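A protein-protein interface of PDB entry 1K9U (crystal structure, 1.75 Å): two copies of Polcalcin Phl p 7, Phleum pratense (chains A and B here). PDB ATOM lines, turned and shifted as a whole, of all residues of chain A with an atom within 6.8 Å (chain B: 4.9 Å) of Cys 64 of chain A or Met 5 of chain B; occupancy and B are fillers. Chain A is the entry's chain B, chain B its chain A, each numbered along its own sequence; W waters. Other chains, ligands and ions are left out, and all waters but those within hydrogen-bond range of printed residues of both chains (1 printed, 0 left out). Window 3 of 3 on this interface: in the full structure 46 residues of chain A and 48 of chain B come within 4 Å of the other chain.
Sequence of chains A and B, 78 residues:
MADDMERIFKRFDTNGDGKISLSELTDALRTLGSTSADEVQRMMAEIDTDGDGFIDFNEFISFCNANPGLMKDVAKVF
NH1 of Arg 7 of chain B lies within salt-bridge range of OD1 of Asp 4 of chain B (2.6 Å). O of Phe 60 of chain A sits at hydrogen-bond distance from SG of Cys 64 of chain A (3.3 Å). OD1 of Asp 3 of chain B lies within hydrogen-bond range of N of Met 5 of chain B (3.1 Å).
N of Phe 57 of chain A touches CZ of Phe 9 of chain B (3.6 Å). Phe 60 of chain A touches Met 5 of chain B. Phe 60 of chain A touches Phe 9 of chain B. Cys 64 of chain A touches Met 5 of chain B (CB to SD, 3.8 Å). CE of Met 71 of chain A touches OD2 of Asp 4 of chain B, 2.9 Å away. Met 5 of chain B touches Met 71 of chain A.
Of the printed residues of chain B, Phe 57 of chain A touches Phe 9. Of the printed residues of chain B, Phe 60 of chain A touches Met 5 and Phe 9. Printed residues of chain B within 4 Å of Cys 64 of chain A: Met 5. Printed residues of chain B within 4 Å of Met 71 of chain A: Asp 4 and Met 5. Of the printed residues of chain A, Asp 4 of chain B touches Met 71 (2.9 Å). Printed residues of chain A within 4 Å of Met 5 of chain B: Phe 60, Cys 64 and Met 71. Printed residues of chain A within 4 Å of Phe 9 of chain B: Phe 57 (3.6 Å) and Phe 60 (3.8 Å). The nearest printed residue of chain B that does not touch Phe 60 of chain A is Ile 8 of chain B (4.3 Å).
Of the 7 printed residues of chain B, 3 touch a printed residue of chain A. Printed residues of chain B that touch a printed residue of chain A: Asp 4, Met 5 and Phe 9. Hydrophobic or aromatic side chains of chain B that line the printed part of chain A: Met 5 and Phe 9. Of the 15 printed residues of chain A, 4 touch a printed residue of chain B. Printed residues of chain A that touch a printed residue of chain B: Phe 57, Phe 60, Cys 64 and Met 71. Hydrophobic or aromatic side chains of chain A that line the printed part of chain B: Phe 57, Phe 60 and Met 71. Among the printed residues, 6 pairs touch across the chains. Among the printed residues, no Asp or Glu carboxylate lies within 4 Å of a Lys or Arg side-chain nitrogen of the other chain.
No position is printed for both chains. Of the 6 pairs that touch across the chains among the printed residues, none has its exchanged pair printed and touching as well.
Water W1 lies within hydrogen-bond range of O of Met 71 of chain A and OD2 of Asp 4 of chain B.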
ATOM      1  N   ILE A  47       6.523 -10.769 -29.467  1.00  0.00           N
ATOM      2  CA  ILE A  47       7.927 -10.742 -29.070  1.00  0.00           C
ATOM      3  C   ILE A  47       8.691 -12.044 -29.334  1.00  0.00           C
ATOM      4  O   ILE A  47       9.910 -12.026 -29.498  1.00  0.00           O
ATOM      5  CB  ILE A  47       8.043 -10.348 -27.569  1.00  0.00           C
ATOM      6  CG1 ILE A  47       9.505 -10.128 -27.182  1.00  0.00           C
ATOM      7  CG2 ILE A  47       7.427 -11.426 -26.706  1.00  0.00           C
ATOM      8  CD1 ILE A  47       9.683  -9.486 -25.814  1.00  0.00           C
ATOM      9  N   PHE A  57      16.422 -14.184 -23.817  1.00  0.00           N
ATOM     10  CA  PHE A  57      17.088 -12.904 -23.633  1.00  0.00           C
ATOM     11  C   PHE A  57      17.369 -12.176 -24.944  1.00  0.00           C
ATOM     12  O   PHE A  57      17.263 -10.955 -25.000  1.00  0.00           O
ATOM     13  CB  PHE A  57      18.372 -13.090 -22.817  1.00  0.00           C
ATOM     14  CG  PHE A  57      18.881 -11.820 -22.183  1.00  0.00           C
ATOM     15  CD1 PHE A  57      18.013 -10.964 -21.502  1.00  0.00           C
ATOM     16  CD2 PHE A  57      20.232 -11.498 -22.235  1.00  0.00           C
ATOM     17  CE1 PHE A  57      18.487  -9.803 -20.884  1.00  0.00           C
ATOM     18  CE2 PHE A  57      20.719 -10.344 -21.621  1.00  0.00           C
ATOM     19  CZ  PHE A  57      19.847  -9.495 -20.944  1.00  0.00           C
ATOM     20  N   GLU A  59      15.574 -12.207 -27.642  1.00  0.00           N
ATOM     21  CA  GLU A  59      14.308 -11.619 -28.055  1.00  0.00           C
ATOM     22  C   GLU A  59      13.931 -10.435 -27.176  1.00  0.00           C
ATOM     23  O   GLU A  59      13.395  -9.445 -27.670  1.00  0.00           O
ATOM     24  CB  GLU A  59      13.210 -12.685 -28.040  1.00  0.00           C
ATOM     25  CG  GLU A  59      13.475 -13.804 -29.058  1.00  0.00           C
ATOM     26  CD  GLU A  59      12.570 -15.003 -28.885  1.00  0.00           C
ATOM     27  OE1 GLU A  59      12.195 -15.308 -27.737  1.00  0.00           O
ATOM     28  OE2 GLU A  59      12.246 -15.658 -29.895  1.00  0.00           O
ATOM     29  N   PHE A  60      14.227 -10.527 -25.881  1.00  0.00           N
ATOM     30  CA  PHE A  60      13.918  -9.429 -24.970  1.00  0.00           C
ATOM     31  C   PHE A  60      14.756  -8.201 -25.331  1.00  0.00           C
ATOM     32  O   PHE A  60      14.244  -7.088 -25.389  1.00  0.00           O
ATOM     33  CB  PHE A  60      14.192  -9.828 -23.519  1.00  0.00           C
ATOM     34  CG  PHE A  60      13.800  -8.771 -22.526  1.00  0.00           C
ATOM     35  CD1 PHE A  60      12.478  -8.344 -22.435  1.00  0.00           C
ATOM     36  CD2 PHE A  60      14.750  -8.186 -21.699  1.00  0.00           C
ATOM     37  CE1 PHE A  60      12.111  -7.344 -21.529  1.00  0.00           C
ATOM     38  CE2 PHE A  60      14.392  -7.192 -20.792  1.00  0.00           C
ATOM     39  CZ  PHE A  60      13.075  -6.771 -20.709  1.00  0.00           C
ATOM     40  N   ILE A  61      16.044  -8.413 -25.582  1.00  0.00           N
ATOM     41  CA  ILE A  61      16.938  -7.321 -25.955  1.00  0.00           C
ATOM     42  C   ILE A  61      16.477  -6.668 -27.258  1.00  0.00           C
ATOM     43  O   ILE A  61      16.427  -5.440 -27.365  1.00  0.00           O
ATOM     44  CB  ILE A  61      18.385  -7.827 -26.134  1.00  0.00           C
ATOM     45  CG1 ILE A  61      18.950  -8.252 -24.777  1.00  0.00           C
ATOM     46  CG2 ILE A  61      19.253  -6.736 -26.768  1.00  0.00           C
ATOM     47  CD1 ILE A  61      20.299  -8.939 -24.866  1.00  0.00           C
ATOM     48  N   SER A  62      16.149  -7.491 -28.248  1.00  0.00           N
ATOM     49  CA  SER A  62      15.694  -6.988 -29.537  1.00  0.00           C
ATOM     50  C   SER A  62      14.452  -6.119 -29.364  1.00  0.00           C
ATOM     51  O   SER A  62      14.346  -5.043 -29.952  1.00  0.00           O
ATOM     52  CB  SER A  62      15.381  -8.152 -30.484  1.00  0.00           C
ATOM     53  OG  SER A  62      16.537  -8.928 -30.745  1.00  0.00           O
ATOM     54  N   PHE A  63      13.515  -6.593 -28.548  1.00  0.00           N
ATOM     55  CA  PHE A  63      12.285  -5.858 -28.299  1.00  0.00           C
ATOM     56  C   PHE A  63      12.605  -4.529 -27.612  1.00  0.00           C
ATOM     57  O   PHE A  63      12.037  -3.492 -27.949  1.00  0.00           O
ATOM     58  CB  PHE A  63      11.348  -6.688 -27.422  1.00  0.00           C
ATOM     59  CG  PHE A  63       9.957  -6.144 -27.349  1.00  0.00           C
ATOM     60  CD1 PHE A  63       9.080  -6.308 -28.414  1.00  0.00           C
ATOM     61  CD2 PHE A  63       9.535  -5.434 -26.234  1.00  0.00           C
ATOM     62  CE1 PHE A  63       7.791  -5.771 -28.368  1.00  0.00           C
ATOM     63  CE2 PHE A  63       8.248  -4.894 -26.177  1.00  0.00           C
ATOM     64  CZ  PHE A  63       7.379  -5.064 -27.249  1.00  0.00           C
ATOM     65  N   CYS A  64      13.520  -4.564 -26.647  1.00  0.00           N
ATOM     66  CA  CYS A  64      13.909  -3.354 -25.941  1.00  0.00           C
ATOM     67  C   CYS A  64      14.561  -2.357 -26.895  1.00  0.00           C
ATOM     68  O   CYS A  64      14.292  -1.158 -26.822  1.00  0.00           O
ATOM     69  CB  CYS A  64      14.872  -3.682 -24.795  1.00  0.00           C
ATOM     70  SG  CYS A  64      14.079  -4.465 -23.369  1.00  0.00           S
ATOM     71  N   ASN A  65      15.415  -2.846 -27.793  1.00  0.00           N
ATOM     72  CA  ASN A  65      16.074  -1.952 -28.744  1.00  0.00           C
ATOM     73  C   ASN A  65      15.062  -1.280 -29.672  1.00  0.00           C
ATOM     74  O   ASN A  65      15.250  -0.135 -30.072  1.00  0.00           O
ATOM     75  CB  ASN A  65      17.110  -2.705 -29.588  1.00  0.00           C
ATOM     76  CG  ASN A  65      18.336  -3.110 -28.790  1.00  0.00           C
ATOM     77  OD1 ASN A  65      18.679  -2.480 -27.787  1.00  0.00           O
ATOM     78  ND2 ASN A  65      19.020  -4.155 -29.249  1.00  0.00           N
ATOM     79  N   ALA A  66      13.991  -1.992 -30.012  1.00  0.00           N
ATOM     80  CA  ALA A  66      12.964  -1.441 -30.895  1.00  0.00           C
ATOM     81  C   ALA A  66      11.963  -0.579 -30.127  1.00  0.00           C
ATOM     82  O   ALA A  66      11.233   0.220 -30.717  1.00  0.00           O
ATOM     83  CB  ALA A  66      12.233  -2.568 -31.615  1.00  0.00           C
ATOM     84  N   ASN A  67      11.945  -0.743 -28.808  1.00  0.00           N
ATOM     85  CA  ASN A  67      11.030  -0.009 -27.933  1.00  0.00           C
ATOM     86  C   ASN A  67      11.796   0.534 -26.732  1.00  0.00           C
ATOM     87  O   ASN A  67      11.692   0.005 -25.624  1.00  0.00           O
ATOM     88  CB  ASN A  67       9.921  -0.946 -27.450  1.00  0.00           C
ATOM     89  CG  ASN A  67       9.107  -1.513 -28.586  1.00  0.00           C
ATOM     90  OD1 ASN A  67       8.138  -0.902 -29.040  1.00  0.00           O
ATOM     91  ND2 ASN A  67       9.507  -2.682 -29.070  1.00  0.00           N
ATOM     92  N   PRO A  68      12.578   1.604 -26.939  1.00  0.00           N
ATOM     93  CA  PRO A  68      13.371   2.220 -25.874  1.00  0.00           C
ATOM     94  C   PRO A  68      12.560   2.641 -24.655  1.00  0.00           C
ATOM     95  O   PRO A  68      13.098   2.763 -23.558  1.00  0.00           O
ATOM     96  CB  PRO A  68      14.034   3.402 -26.577  1.00  0.00           C
ATOM     97  CG  PRO A  68      13.051   3.759 -27.646  1.00  0.00           C
ATOM     98  CD  PRO A  68      12.656   2.400 -28.176  1.00  0.00           C
ATOM     99  N   GLY A  69      11.264   2.854 -24.859  1.00  0.00           N
ATOM    100  CA  GLY A  69      10.396   3.265 -23.770  1.00  0.00           C
ATOM    101  C   GLY A  69      10.140   2.170 -22.756  1.00  0.00           C
ATOM    102  O   GLY A  69       9.711   2.446 -21.638  1.00  0.00           O
ATOM    103  N   LEU A  70      10.396   0.921 -23.131  1.00  0.00           N
ATOM    104  CA  LEU A  70      10.168  -0.176 -22.203  1.00  0.00           C
ATOM    105  C   LEU A  70      11.093  -0.066 -21.000  1.00  0.00           C
ATOM    106  O   LEU A  70      10.649  -0.161 -19.855  1.00  0.00           O
ATOM    107  CB  LEU A  70      10.378  -1.528 -22.891  1.00  0.00           C
ATOM    108  CG  LEU A  70      10.122  -2.750 -22.002  1.00  0.00           C
ATOM    109  CD1 LEU A  70       8.709  -2.685 -21.435  1.00  0.00           C
ATOM    110  CD2 LEU A  70      10.313  -4.027 -22.814  1.00  0.00           C
ATOM    111  N   MET A  71      12.379   0.144 -21.259  1.00  0.00           N
ATOM    112  CA  MET A  71      13.356   0.257 -20.183  1.00  0.00           C
ATOM    113  C   MET A  71      13.463   1.665 -19.609  1.00  0.00           C
ATOM    114  O   MET A  71      13.701   1.833 -18.415  1.00  0.00           O
ATOM    115  CB  MET A  71      14.736  -0.197 -20.671  1.00  0.00           C
ATOM    116  CG  MET A  71      14.836  -1.685 -20.963  1.00  0.00           C
ATOM    117  SD  MET A  71      14.342  -2.681 -19.546  1.00  0.00           S
ATOM    118  CE  MET A  71      15.488  -2.137 -18.373  1.00  0.00           C
ATOM    119  N   ASP B   3      22.543  -4.240 -15.790  1.00  0.00           N
ATOM    120  CA  ASP B   3      21.610  -3.100 -16.001  1.00  0.00           C
ATOM    121  C   ASP B   3      20.184  -3.520 -15.687  1.00  0.00           C
ATOM    122  O   ASP B   3      19.937  -4.655 -15.282  1.00  0.00           O
ATOM    123  CB  ASP B   3      21.695  -2.597 -17.446  1.00  0.00           C
ATOM    124  CG  ASP B   3      21.264  -3.640 -18.463  1.00  0.00           C
ATOM    125  OD1 ASP B   3      20.858  -4.751 -18.060  1.00  0.00           O
ATOM    126  OD2 ASP B   3      21.329  -3.339 -19.673  1.00  0.00           O
ATOM    127  N   ASP B   4      19.246  -2.602 -15.881  1.00  0.00           N
ATOM    128  CA  ASP B   4      17.848  -2.885 -15.600  1.00  0.00           C
ATOM    129  C   ASP B   4      17.253  -3.921 -16.556  1.00  0.00           C
ATOM    130  O   ASP B   4      16.276  -4.585 -16.220  1.00  0.00           O
ATOM    131  CB  ASP B   4      17.033  -1.589 -15.653  1.00  0.00           C
ATOM    132  CG  ASP B   4      15.665  -1.735 -15.015  1.00  0.00           C
ATOM    133  OD1 ASP B   4      15.606  -2.096 -13.821  1.00  0.00           O
ATOM    134  OD2 ASP B   4      14.650  -1.485 -15.700  1.00  0.00           O
ATOM    135  N   MET B   5      17.836  -4.057 -17.745  1.00  0.00           N
ATOM    136  CA  MET B   5      17.338  -5.035 -18.714  1.00  0.00           C
ATOM    137  C   MET B   5      17.492  -6.443 -18.164  1.00  0.00           C
ATOM    138  O   MET B   5      16.524  -7.197 -18.075  1.00  0.00           O
ATOM    139  CB  MET B   5      18.096  -4.951 -20.045  1.00  0.00           C
ATOM    140  CG  MET B   5      17.659  -3.832 -20.973  1.00  0.00           C
ATOM    141  SD  MET B   5      17.977  -4.238 -22.712  1.00  0.00           S
ATOM    142  CE  MET B   5      19.770  -4.174 -22.766  1.00  0.00           C
ATOM    143  N   GLU B   6      18.721  -6.790 -17.799  1.00  0.00           N
ATOM    144  CA  GLU B   6      19.011  -8.116 -17.268  1.00  0.00           C
ATOM    145  C   GLU B   6      18.249  -8.292 -15.958  1.00  0.00           C
ATOM    146  O   GLU B   6      17.710  -9.363 -15.680  1.00  0.00           O
ATOM    147  CB  GLU B   6      20.517  -8.250 -17.023  1.00  0.00           C
ATOM    148  CG  GLU B   6      21.042  -9.663 -16.786  1.00  0.00           C
ATOM    149  CD  GLU B   6      20.546 -10.283 -15.495  1.00  0.00           C
ATOM    150  OE1 GLU B   6      20.450  -9.557 -14.483  1.00  0.00           O
ATOM    151  OE2 GLU B   6      20.270 -11.502 -15.489  1.00  0.00           O
ATOM    152  N   ARG B   7      18.202  -7.227 -15.162  1.00  0.00           N
ATOM    153  CA  ARG B   7      17.512  -7.257 -13.876  1.00  0.00           C
ATOM    154  C   ARG B   7      16.029  -7.556 -14.030  1.00  0.00           C
ATOM    155  O   ARG B   7      15.485  -8.400 -13.318  1.00  0.00           O
ATOM    156  CB  ARG B   7      17.685  -5.924 -13.142  1.00  0.00           C
ATOM    157  CG  ARG B   7      19.107  -5.620 -12.707  1.00  0.00           C
ATOM    158  CD  ARG B   7      19.243  -4.220 -12.105  1.00  0.00           C
ATOM    159  NE  ARG B   7      18.454  -4.043 -10.886  1.00  0.00           N
ATOM    160  CZ  ARG B   7      17.148  -3.789 -10.857  1.00  0.00           C
ATOM    161  NH1 ARG B   7      16.462  -3.676 -11.985  1.00  0.00           N
ATOM    162  NH2 ARG B   7      16.525  -3.652  -9.695  1.00  0.00           N
ATOM    163  N   ILE B   8      15.380  -6.851 -14.955  1.00  0.00           N
ATOM    164  CA  ILE B   8      13.952  -7.033 -15.212  1.00  0.00           C
ATOM    165  C   ILE B   8      13.674  -8.423 -15.779  1.00  0.00           C
ATOM    166  O   ILE B   8      12.708  -9.080 -15.393  1.00  0.00           O
ATOM    167  CB  ILE B   8      13.418  -5.975 -16.217  1.00  0.00           C
ATOM    168  CG1 ILE B   8      13.507  -4.574 -15.601  1.00  0.00           C
ATOM    169  CG2 ILE B   8      11.977  -6.290 -16.598  1.00  0.00           C
ATOM    170  CD1 ILE B   8      12.688  -4.399 -14.341  1.00  0.00           C
ATOM    171  N   PHE B   9      14.522  -8.867 -16.702  1.00  0.00           N
ATOM    172  CA  PHE B   9      14.350 -10.186 -17.309  1.00  0.00           C
ATOM    173  C   PHE B   9      14.412 -11.261 -16.226  1.00  0.00           C
ATOM    174  O   PHE B   9      13.566 -12.154 -16.164  1.00  0.00           O
ATOM    175  CB  PHE B   9      15.449 -10.438 -18.345  1.00  0.00           C
ATOM    176  CG  PHE B   9      15.257 -11.703 -19.134  1.00  0.00           C
ATOM    177  CD1 PHE B   9      14.402 -11.731 -20.236  1.00  0.00           C
ATOM    178  CD2 PHE B   9      15.918 -12.872 -18.767  1.00  0.00           C
ATOM    179  CE1 PHE B   9      14.207 -12.908 -20.960  1.00  0.00           C
ATOM    180  CE2 PHE B   9      15.730 -14.058 -19.483  1.00  0.00           C
ATOM    181  CZ  PHE B   9      14.872 -14.075 -20.582  1.00  0.00           C
HETATM  182  O   HOH W   1      14.856   1.454 -16.150  1.00  0.00           O
